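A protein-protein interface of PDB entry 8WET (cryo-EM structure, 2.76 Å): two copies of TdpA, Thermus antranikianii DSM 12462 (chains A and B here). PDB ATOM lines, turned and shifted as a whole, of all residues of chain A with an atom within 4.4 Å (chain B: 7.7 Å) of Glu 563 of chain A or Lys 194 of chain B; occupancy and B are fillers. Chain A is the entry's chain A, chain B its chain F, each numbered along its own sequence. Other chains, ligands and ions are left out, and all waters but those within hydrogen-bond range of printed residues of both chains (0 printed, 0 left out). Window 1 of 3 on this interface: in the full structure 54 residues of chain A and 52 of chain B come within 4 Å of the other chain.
The side-chain carboxylate (OE2) of Glu 563 of chain A lies within salt-bridge range of the side-chain amino group (NZ) of Lys 194 of chain B. The side-chain hydroxyl (OH) of Tyr 565 of chain A sits at hydrogen-bond distance from the backbone carbonyl oxygen (O) of Gly 196 of chain B (3.1 Å).
O of Glu 519 of chain A is in hydrogen-bond range of N of Glu 563 of chain A, 2.9 Å away. O of His 525 of chain B lies within hydrogen-bond range of N of Lys 194 of chain B, at 3.0 Å.
Among the printed residues, pairs that only touch across the chains: Pro 564 of chain A with Phe 197 of chain B.
Glu 563 of chain A touches just one residue of chain B: Lys 194 (3.3 Å). Of the printed residues of chain B, Pro 564 of chain A touches Phe 197. Of the printed residues of chain B, Tyr 565 of chain A touches Gly 196. Lys 194 of chain B touches just one residue of chain A: Glu 563 (3.3 Å). Printed residues of chain A within 4 Å of Gly 196 of chain B: Tyr 565 (3.1 Å). Printed residues of chain A within 4 Å of Phe 197 of chain B: Pro 564 (3.9 Å). The nearest printed residue of chain B that does not touch Pro 564 of chain A is Thr 195 of chain B (4.1 Å).
Printed residues of chain A that touch a printed residue of chain B: Glu 563, Pro 564 and Tyr 565. Of the 21 printed residues of chain B, 3 touch a printed residue of chain A. Hydrophobic or aromatic side chains of chain B within 4 Å of the printed part of chain A: Phe 197. Among the printed residues, 3 pairs touch across the chains. Among the printed residues, Asp or Glu carboxylates within 4 Å of a Lys or Arg side-chain nitrogen of the other chain: Glu 563 of chain A with Lys 194 of chain B (3.3 Å).
No position is printed for both chains. Of the 3 pairs that touch across the chains among the printed residues, none has its exchanged pair printed and touching as well.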
ATOM      1  N   ARG A 187      11.710   6.081   5.123  1.00  0.00           N
ATOM      2  CA  ARG A 187      12.756   5.223   4.590  1.00  0.00           C
ATOM      3  C   ARG A 187      13.594   4.660   5.733  1.00  0.00           C
ATOM      4  O   ARG A 187      13.442   5.043   6.894  1.00  0.00           O
ATOM      5  CB  ARG A 187      13.631   5.994   3.595  1.00  0.00           C
ATOM      6  CG  ARG A 187      12.837   6.578   2.436  1.00  0.00           C
ATOM      7  CD  ARG A 187      13.672   7.489   1.558  1.00  0.00           C
ATOM      8  NE  ARG A 187      14.678   6.759   0.798  1.00  0.00           N
ATOM      9  CZ  ARG A 187      15.549   7.328  -0.023  1.00  0.00           C
ATOM     10  NH1 ARG A 187      15.554   8.634  -0.227  1.00  0.00           N
ATOM     11  NH2 ARG A 187      16.434   6.568  -0.660  1.00  0.00           N
ATOM     12  N   THR A 518      17.549  -1.482   2.849  1.00  0.00           N
ATOM     13  CA  THR A 518      17.910  -0.183   3.396  1.00  0.00           C
ATOM     14  C   THR A 518      18.335   0.767   2.280  1.00  0.00           C
ATOM     15  O   THR A 518      18.949   0.364   1.289  1.00  0.00           O
ATOM     16  CB  THR A 518      19.037  -0.330   4.418  1.00  0.00           C
ATOM     17  OG1 THR A 518      18.775  -1.460   5.258  1.00  0.00           O
ATOM     18  CG2 THR A 518      19.141   0.912   5.285  1.00  0.00           C
ATOM     19  N   GLU A 519      17.996   2.044   2.452  1.00  0.00           N
ATOM     20  CA  GLU A 519      18.293   3.071   1.461  1.00  0.00           C
ATOM     21  C   GLU A 519      19.514   3.908   1.824  1.00  0.00           C
ATOM     22  O   GLU A 519      20.402   4.098   0.990  1.00  0.00           O
ATOM     23  CB  GLU A 519      17.078   3.988   1.272  1.00  0.00           C
ATOM     24  CG  GLU A 519      15.870   3.316   0.639  1.00  0.00           C
ATOM     25  CD  GLU A 519      14.967   2.660   1.662  1.00  0.00           C
ATOM     26  OE1 GLU A 519      15.245   2.786   2.871  1.00  0.00           O
ATOM     27  OE2 GLU A 519      13.974   2.020   1.259  1.00  0.00           O
ATOM     28  N   LYS A 539      25.813  -3.739  -1.055  1.00  0.00           N
ATOM     29  CA  LYS A 539      25.970  -2.549  -1.887  1.00  0.00           C
ATOM     30  C   LYS A 539      27.328  -2.600  -2.575  1.00  0.00           C
ATOM     31  O   LYS A 539      28.367  -2.533  -1.911  1.00  0.00           O
ATOM     32  CB  LYS A 539      25.829  -1.276  -1.053  1.00  0.00           C
ATOM     33  CG  LYS A 539      24.521  -1.184  -0.288  1.00  0.00           C
ATOM     34  CD  LYS A 539      23.389  -0.738  -1.193  1.00  0.00           C
ATOM     35  CE  LYS A 539      22.054  -0.792  -0.474  1.00  0.00           C
ATOM     36  NZ  LYS A 539      21.504  -2.175  -0.432  1.00  0.00           N
ATOM     37  N   TYR A 561      25.990   7.117   1.777  1.00  0.00           N
ATOM     38  CA  TYR A 561      25.459   6.655   0.499  1.00  0.00           C
ATOM     39  C   TYR A 561      23.945   6.615   0.607  1.00  0.00           C
ATOM     40  O   TYR A 561      23.404   5.835   1.395  1.00  0.00           O
ATOM     41  CB  TYR A 561      26.013   5.277   0.140  1.00  0.00           C
ATOM     42  CG  TYR A 561      25.647   4.820  -1.252  1.00  0.00           C
ATOM     43  CD1 TYR A 561      26.137   5.478  -2.369  1.00  0.00           C
ATOM     44  CD2 TYR A 561      24.809   3.731  -1.446  1.00  0.00           C
ATOM     45  CE1 TYR A 561      25.806   5.067  -3.640  1.00  0.00           C
ATOM     46  CE2 TYR A 561      24.472   3.312  -2.716  1.00  0.00           C
ATOM     47  CZ  TYR A 561      24.973   3.983  -3.809  1.00  0.00           C
ATOM     48  OH  TYR A 561      24.641   3.570  -5.078  1.00  0.00           O
ATOM     49  N   PHE A 562      23.265   7.451  -0.173  1.00  0.00           N
ATOM     50  CA  PHE A 562      21.810   7.551  -0.152  1.00  0.00           C
ATOM     51  C   PHE A 562      21.265   6.991  -1.459  1.00  0.00           C
ATOM     52  O   PHE A 562      21.440   7.595  -2.521  1.00  0.00           O
ATOM     53  CB  PHE A 562      21.367   8.997   0.055  1.00  0.00           C
ATOM     54  CG  PHE A 562      22.033   9.675   1.217  1.00  0.00           C
ATOM     55  CD1 PHE A 562      21.917   9.161   2.497  1.00  0.00           C
ATOM     56  CD2 PHE A 562      22.776  10.826   1.031  1.00  0.00           C
ATOM     57  CE1 PHE A 562      22.529   9.784   3.566  1.00  0.00           C
ATOM     58  CE2 PHE A 562      23.390  11.451   2.096  1.00  0.00           C
ATOM     59  CZ  PHE A 562      23.266  10.929   3.365  1.00  0.00           C
ATOM     60  N   GLU A 563      20.598   5.844  -1.375  1.00  0.00           N
ATOM     61  CA  GLU A 563      20.017   5.211  -2.543  1.00  0.00           C
ATOM     62  C   GLU A 563      18.794   5.994  -3.021  1.00  0.00           C
ATOM     63  O   GLU A 563      18.185   6.740  -2.251  1.00  0.00           O
ATOM     64  CB  GLU A 563      19.635   3.770  -2.220  1.00  0.00           C
ATOM     65  CG  GLU A 563      20.798   2.801  -2.286  1.00  0.00           C
ATOM     66  CD  GLU A 563      20.365   1.408  -2.687  1.00  0.00           C
ATOM     67  OE1 GLU A 563      19.189   1.059  -2.453  1.00  0.00           O
ATOM     68  OE2 GLU A 563      21.198   0.663  -3.242  1.00  0.00           O
ATOM     69  N   PRO A 564      18.408   5.837  -4.299  1.00  0.00           N
ATOM     70  CA  PRO A 564      19.008   5.003  -5.343  1.00  0.00           C
ATOM     71  C   PRO A 564      19.755   5.778  -6.423  1.00  0.00           C
ATOM     72  O   PRO A 564      20.199   5.182  -7.397  1.00  0.00           O
ATOM     73  CB  PRO A 564      17.782   4.295  -5.928  1.00  0.00           C
ATOM     74  CG  PRO A 564      16.647   5.307  -5.771  1.00  0.00           C
ATOM     75  CD  PRO A 564      17.086   6.323  -4.727  1.00  0.00           C
ATOM     76  N   TYR A 565      19.918   7.096  -6.296  1.00  0.00           N
ATOM     77  CA  TYR A 565      20.474   7.904  -7.375  1.00  0.00           C
ATOM     78  C   TYR A 565      21.797   8.569  -7.017  1.00  0.00           C
ATOM     79  O   TYR A 565      22.238   9.465  -7.744  1.00  0.00           O
ATOM     80  CB  TYR A 565      19.460   8.963  -7.813  1.00  0.00           C
ATOM     81  CG  TYR A 565      18.155   8.385  -8.306  1.00  0.00           C
ATOM     82  CD1 TYR A 565      18.136   7.277  -9.139  1.00  0.00           C
ATOM     83  CD2 TYR A 565      16.942   8.945  -7.937  1.00  0.00           C
ATOM     84  CE1 TYR A 565      16.947   6.744  -9.591  1.00  0.00           C
ATOM     85  CE2 TYR A 565      15.748   8.420  -8.383  1.00  0.00           C
ATOM     86  CZ  TYR A 565      15.757   7.318  -9.210  1.00  0.00           C
ATOM     87  OH  TYR A 565      14.568   6.792  -9.657  1.00  0.00           O
ATOM     88  N   ASN B 191      11.649 -10.196 -14.529  1.00  0.00           N
ATOM     89  CA  ASN B 191      11.999  -8.779 -14.542  1.00  0.00           C
ATOM     90  C   ASN B 191      13.019  -8.521 -13.439  1.00  0.00           C
ATOM     91  O   ASN B 191      12.672  -8.510 -12.253  1.00  0.00           O
ATOM     92  CB  ASN B 191      10.758  -7.906 -14.361  1.00  0.00           C
ATOM     93  CG  ASN B 191      10.799  -6.653 -15.212  1.00  0.00           C
ATOM     94  OD1 ASN B 191      11.856  -6.051 -15.399  1.00  0.00           O
ATOM     95  ND2 ASN B 191       9.648  -6.253 -15.733  1.00  0.00           N
ATOM     96  N   PHE B 192      14.268  -8.296 -13.832  1.00  0.00           N
ATOM     97  CA  PHE B 192      15.363  -8.085 -12.898  1.00  0.00           C
ATOM     98  C   PHE B 192      15.857  -6.647 -12.978  1.00  0.00           C
ATOM     99  O   PHE B 192      15.748  -5.990 -14.015  1.00  0.00           O
ATOM    100  CB  PHE B 192      16.520  -9.046 -13.177  1.00  0.00           C
ATOM    101  CG  PHE B 192      16.145 -10.495 -13.079  1.00  0.00           C
ATOM    102  CD1 PHE B 192      15.243 -10.929 -12.125  1.00  0.00           C
ATOM    103  CD2 PHE B 192      16.697 -11.425 -13.940  1.00  0.00           C
ATOM    104  CE1 PHE B 192      14.897 -12.263 -12.034  1.00  0.00           C
ATOM    105  CE2 PHE B 192      16.357 -12.759 -13.852  1.00  0.00           C
ATOM    106  CZ  PHE B 192      15.457 -13.178 -12.897  1.00  0.00           C
ATOM    107  N   GLY B 193      16.405  -6.172 -11.874  1.00  0.00           N
ATOM    108  CA  GLY B 193      16.881  -4.807 -11.751  1.00  0.00           C
ATOM    109  C   GLY B 193      16.460  -4.230 -10.415  1.00  0.00           C
ATOM    110  O   GLY B 193      15.493  -4.665  -9.791  1.00  0.00           O
ATOM    111  N   LYS B 194      17.205  -3.224  -9.966  1.00  0.00           N
ATOM    112  CA  LYS B 194      16.910  -2.616  -8.680  1.00  0.00           C
ATOM    113  C   LYS B 194      15.746  -1.634  -8.802  1.00  0.00           C
ATOM    114  O   LYS B 194      15.349  -1.224  -9.895  1.00  0.00           O
ATOM    115  CB  LYS B 194      18.147  -1.922  -8.113  1.00  0.00           C
ATOM    116  CG  LYS B 194      18.816  -0.950  -9.061  1.00  0.00           C
ATOM    117  CD  LYS B 194      19.968  -0.233  -8.381  1.00  0.00           C
ATOM    118  CE  LYS B 194      19.516   0.473  -7.116  1.00  0.00           C
ATOM    119  NZ  LYS B 194      20.636   1.207  -6.469  1.00  0.00           N
ATOM    120  N   THR B 195      15.193  -1.266  -7.650  1.00  0.00           N
ATOM    121  CA  THR B 195      13.996  -0.437  -7.612  1.00  0.00           C
ATOM    122  C   THR B 195      14.291   0.968  -8.122  1.00  0.00           C
ATOM    123  O   THR B 195      15.279   1.590  -7.724  1.00  0.00           O
ATOM    124  CB  THR B 195      13.444  -0.374  -6.188  1.00  0.00           C
ATOM    125  OG1 THR B 195      13.387  -1.696  -5.638  1.00  0.00           O
ATOM    126  CG2 THR B 195      12.051   0.232  -6.181  1.00  0.00           C
ATOM    127  N   GLY B 196      13.428   1.465  -9.001  1.00  0.00           N
ATOM    128  CA  GLY B 196      13.544   2.811  -9.516  1.00  0.00           C
ATOM    129  C   GLY B 196      14.252   2.957 -10.843  1.00  0.00           C
ATOM    130  O   GLY B 196      14.628   4.079 -11.197  1.00  0.00           O
ATOM    131  N   PHE B 197      14.447   1.869 -11.589  1.00  0.00           N
ATOM    132  CA  PHE B 197      15.174   1.924 -12.853  1.00  0.00           C
ATOM    133  C   PHE B 197      14.338   1.442 -14.036  1.00  0.00           C
ATOM    134  O   PHE B 197      14.892   1.166 -15.104  1.00  0.00           O
ATOM    135  CB  PHE B 197      16.479   1.131 -12.751  1.00  0.00           C
ATOM    136  CG  PHE B 197      17.575   1.868 -12.035  1.00  0.00           C
ATOM    137  CD1 PHE B 197      17.594   1.940 -10.654  1.00  0.00           C
ATOM    138  CD2 PHE B 197      18.581   2.498 -12.744  1.00  0.00           C
ATOM    139  CE1 PHE B 197      18.598   2.624  -9.996  1.00  0.00           C
ATOM    140  CE2 PHE B 197      19.586   3.181 -12.090  1.00  0.00           C
ATOM    141  CZ  PHE B 197      19.595   3.243 -10.716  1.00  0.00           C
ATOM    142  N   GLY B 198      13.021   1.333 -13.874  1.00  0.00           N
ATOM    143  CA  GLY B 198      12.155   1.098 -15.014  1.00  0.00           C
ATOM    144  C   GLY B 198      11.364  -0.195 -15.011  1.00  0.00           C
ATOM    145  O   GLY B 198      10.908  -0.642 -16.066  1.00  0.00           O
ATOM    146  N   LYS B 199      11.192  -0.808 -13.839  1.00  0.00           N
ATOM    147  CA  LYS B 199      10.430  -2.051 -13.762  1.00  0.00           C
ATOM    148  C   LYS B 199       8.949  -1.811 -14.029  1.00  0.00           C
ATOM    149  O   LYS B 199       8.324  -2.528 -14.822  1.00  0.00           O
ATOM    150  CB  LYS B 199      10.634  -2.699 -12.391  1.00  0.00           C
ATOM    151  CG  LYS B 199      10.036  -4.091 -12.250  1.00  0.00           C
ATOM    152  CD  LYS B 199       8.683  -4.055 -11.555  1.00  0.00           C
ATOM    153  CE  LYS B 199       8.800  -3.538 -10.133  1.00  0.00           C
ATOM    154  NZ  LYS B 199       7.466  -3.392  -9.495  1.00  0.00           N
ATOM    155  N   THR B 504      11.795  -9.235  -9.552  1.00  0.00           N
ATOM    156  CA  THR B 504      12.563  -9.295  -8.317  1.00  0.00           C
ATOM    157  C   THR B 504      13.814  -8.441  -8.446  1.00  0.00           C
ATOM    158  O   THR B 504      14.250  -8.096  -9.546  1.00  0.00           O
ATOM    159  CB  THR B 504      12.940 -10.736  -7.944  1.00  0.00           C
ATOM    160  OG1 THR B 504      13.301 -10.792  -6.560  1.00  0.00           O
ATOM    161  CG2 THR B 504      14.109 -11.221  -8.774  1.00  0.00           C
ATOM    162  N   GLN B 505      14.378  -8.096  -7.290  1.00  0.00           N
ATOM    163  CA  GLN B 505      15.615  -7.336  -7.210  1.00  0.00           C
ATOM    164  C   GLN B 505      16.824  -8.211  -6.908  1.00  0.00           C
ATOM    165  O   GLN B 505      17.959  -7.767  -7.108  1.00  0.00           O
ATOM    166  CB  GLN B 505      15.486  -6.245  -6.137  1.00  0.00           C
ATOM    167  CG  GLN B 505      16.598  -5.212  -6.123  1.00  0.00           C
ATOM    168  CD  GLN B 505      16.367  -4.128  -5.089  1.00  0.00           C
ATOM    169  OE1 GLN B 505      15.373  -4.147  -4.365  1.00  0.00           O
ATOM    170  NE2 GLN B 505      17.288  -3.175  -5.015  1.00  0.00           N
ATOM    171  N   SER B 506      16.606  -9.449  -6.458  1.00  0.00           N
ATOM    172  CA  SER B 506      17.670 -10.378  -6.087  1.00  0.00           C
ATOM    173  C   SER B 506      17.500 -11.658  -6.897  1.00  0.00           C
ATOM    174  O   SER B 506      16.900 -12.633  -6.421  1.00  0.00           O
ATOM    175  CB  SER B 506      17.651 -10.673  -4.589  1.00  0.00           C
ATOM    176  OG  SER B 506      17.664  -9.474  -3.834  1.00  0.00           O
ATOM    177  N   PRO B 507      18.003 -11.687  -8.133  1.00  0.00           N
ATOM    178  CA  PRO B 507      17.916 -12.921  -8.932  1.00  0.00           C
ATOM    179  C   PRO B 507      18.637 -14.105  -8.311  1.00  0.00           C
ATOM    180  O   PRO B 507      18.263 -15.253  -8.583  1.00  0.00           O
ATOM    181  CB  PRO B 507      18.551 -12.518 -10.270  1.00  0.00           C
ATOM    182  CG  PRO B 507      18.449 -11.035 -10.315  1.00  0.00           C
ATOM    183  CD  PRO B 507      18.554 -10.561  -8.904  1.00  0.00           C
ATOM    184  N   VAL B 523      16.574  -7.530 -18.181  1.00  0.00           N
ATOM    185  CA  VAL B 523      17.464  -7.252 -17.061  1.00  0.00           C
ATOM    186  C   VAL B 523      17.864  -5.783 -17.079  1.00  0.00           C
ATOM    187  O   VAL B 523      18.209  -5.234 -18.132  1.00  0.00           O
ATOM    188  CB  VAL B 523      18.711  -8.156 -17.099  1.00  0.00           C
ATOM    189  CG1 VAL B 523      19.532  -7.972 -15.837  1.00  0.00           C
ATOM    190  CG2 VAL B 523      18.303  -9.608 -17.265  1.00  0.00           C
ATOM    191  N   LYS B 524      17.823  -5.154 -15.911  1.00  0.00           N
ATOM    192  CA  LYS B 524      18.259  -3.779 -15.718  1.00  0.00           C
ATOM    193  C   LYS B 524      19.445  -3.763 -14.754  1.00  0.00           C
ATOM    194  O   LYS B 524      19.986  -4.808 -14.387  1.00  0.00           O
ATOM    195  CB  LYS B 524      17.104  -2.911 -15.213  1.00  0.00           C
ATOM    196  CG  LYS B 524      16.129  -2.484 -16.294  1.00  0.00           C
ATOM    197  CD  LYS B 524      14.766  -2.167 -15.710  1.00  0.00           C
ATOM    198  CE  LYS B 524      14.083  -3.418 -15.188  1.00  0.00           C
ATOM    199  NZ  LYS B 524      13.556  -4.262 -16.293  1.00  0.00           N
ATOM    200  N   HIS B 525      19.848  -2.560 -14.350  1.00  0.00           N
ATOM    201  CA  HIS B 525      21.022  -2.398 -13.500  1.00  0.00           C
ATOM    202  C   HIS B 525      20.855  -3.146 -12.182  1.00  0.00           C
ATOM    203  O   HIS B 525      19.827  -3.028 -11.511  1.00  0.00           O
ATOM    204  CB  HIS B 525      21.270  -0.913 -13.237  1.00  0.00           C
ATOM    205  CG  HIS B 525      22.294  -0.647 -12.179  1.00  0.00           C
ATOM    206  ND1 HIS B 525      23.603  -1.064 -12.289  1.00  0.00           N
ATOM    207  CD2 HIS B 525      22.203  -0.006 -10.990  1.00  0.00           C
ATOM    208  CE1 HIS B 525      24.273  -0.691 -11.213  1.00  0.00           C
ATOM    209  NE2 HIS B 525      23.446  -0.048 -10.410  1.00  0.00           N
ATOM    210  N   LEU B 526      21.878  -3.916 -11.814  1.00  0.00           N
ATOM    211  CA  LEU B 526      21.896  -4.681 -10.575  1.00  0.00           C
ATOM    212  C   LEU B 526      23.142  -4.318  -9.785  1.00  0.00           C
ATOM    213  O   LEU B 526      24.257  -4.392 -10.311  1.00  0.00           O
ATOM    214  CB  LEU B 526      21.869  -6.189 -10.850  1.00  0.00           C
ATOM    215  CG  LEU B 526      20.594  -6.774 -11.459  1.00  0.00           C
ATOM    216  CD1 LEU B 526      20.887  -8.112 -12.110  1.00  0.00           C
ATOM    217  CD2 LEU B 526      19.516  -6.921 -10.404  1.00  0.00           C
ATOM    218  N   SER B 527      22.956  -3.931  -8.527  1.00  0.00           N
ATOM    219  CA  SER B 527      24.067  -3.541  -7.659  1.00  0.00           C
ATOM    220  C   SER B 527      24.520  -4.718  -6.796  1.00  0.00           C
ATOM    221  O   SER B 527      24.524  -4.658  -5.566  1.00  0.00           O
ATOM    222  CB  SER B 527      23.666  -2.348  -6.797  1.00  0.00           C
ATOM    223  OG  SER B 527      22.462  -2.612  -6.098  1.00  0.00           O
ATOM    224  N   SER B 528      24.913  -5.802  -7.462  1.00  0.00           N
ATOM    225  CA  SER B 528      25.393  -6.992  -6.776  1.00  0.00           C
ATOM    226  C   SER B 528      26.070  -7.904  -7.786  1.00  0.00           C
ATOM    227  O   SER B 528      25.576  -8.068  -8.905  1.00  0.00           O
ATOM    228  CB  SER B 528      24.248  -7.736  -6.078  1.00  0.00           C
ATOM    229  OG  SER B 528      24.739  -8.814  -5.301  1.00  0.00           O
ATOM    230  N   ASP B 531      24.096 -11.609  -8.397  1.00  0.00           N
ATOM    231  CA  ASP B 531      23.001 -11.606  -9.361  1.00  0.00           C
ATOM    232  C   ASP B 531      23.524 -11.696 -10.789  1.00  0.00           C
ATOM    233  O   ASP B 531      22.998 -12.458 -11.608  1.00  0.00           O
ATOM    234  CB  ASP B 531      22.154 -10.348  -9.179  1.00  0.00           C
ATOM    235  CG  ASP B 531      21.731 -10.135  -7.740  1.00  0.00           C
ATOM    236  OD1 ASP B 531      21.655 -11.128  -6.987  1.00  0.00           O
ATOM    237  OD2 ASP B 531      21.471  -8.974  -7.361  1.00  0.00           O
ATOM    238  N   PRO B 553      24.440   2.260 -13.755  1.00  0.00           N
ATOM    239  CA  PRO B 553      23.060   2.605 -13.334  1.00  0.00           C
ATOM    240  C   PRO B 553      22.367   3.607 -14.255  1.00  0.00           C
ATOM    241  O   PRO B 553      22.355   4.818 -14.040  1.00  0.00           O
ATOM    242  CB  PRO B 553      23.273   3.184 -11.933  1.00  0.00           C
ATOM    243  CG  PRO B 553      24.677   3.654 -11.918  1.00  0.00           C
ATOM    244  CD  PRO B 553      25.436   2.684 -12.760  1.00  0.00           C
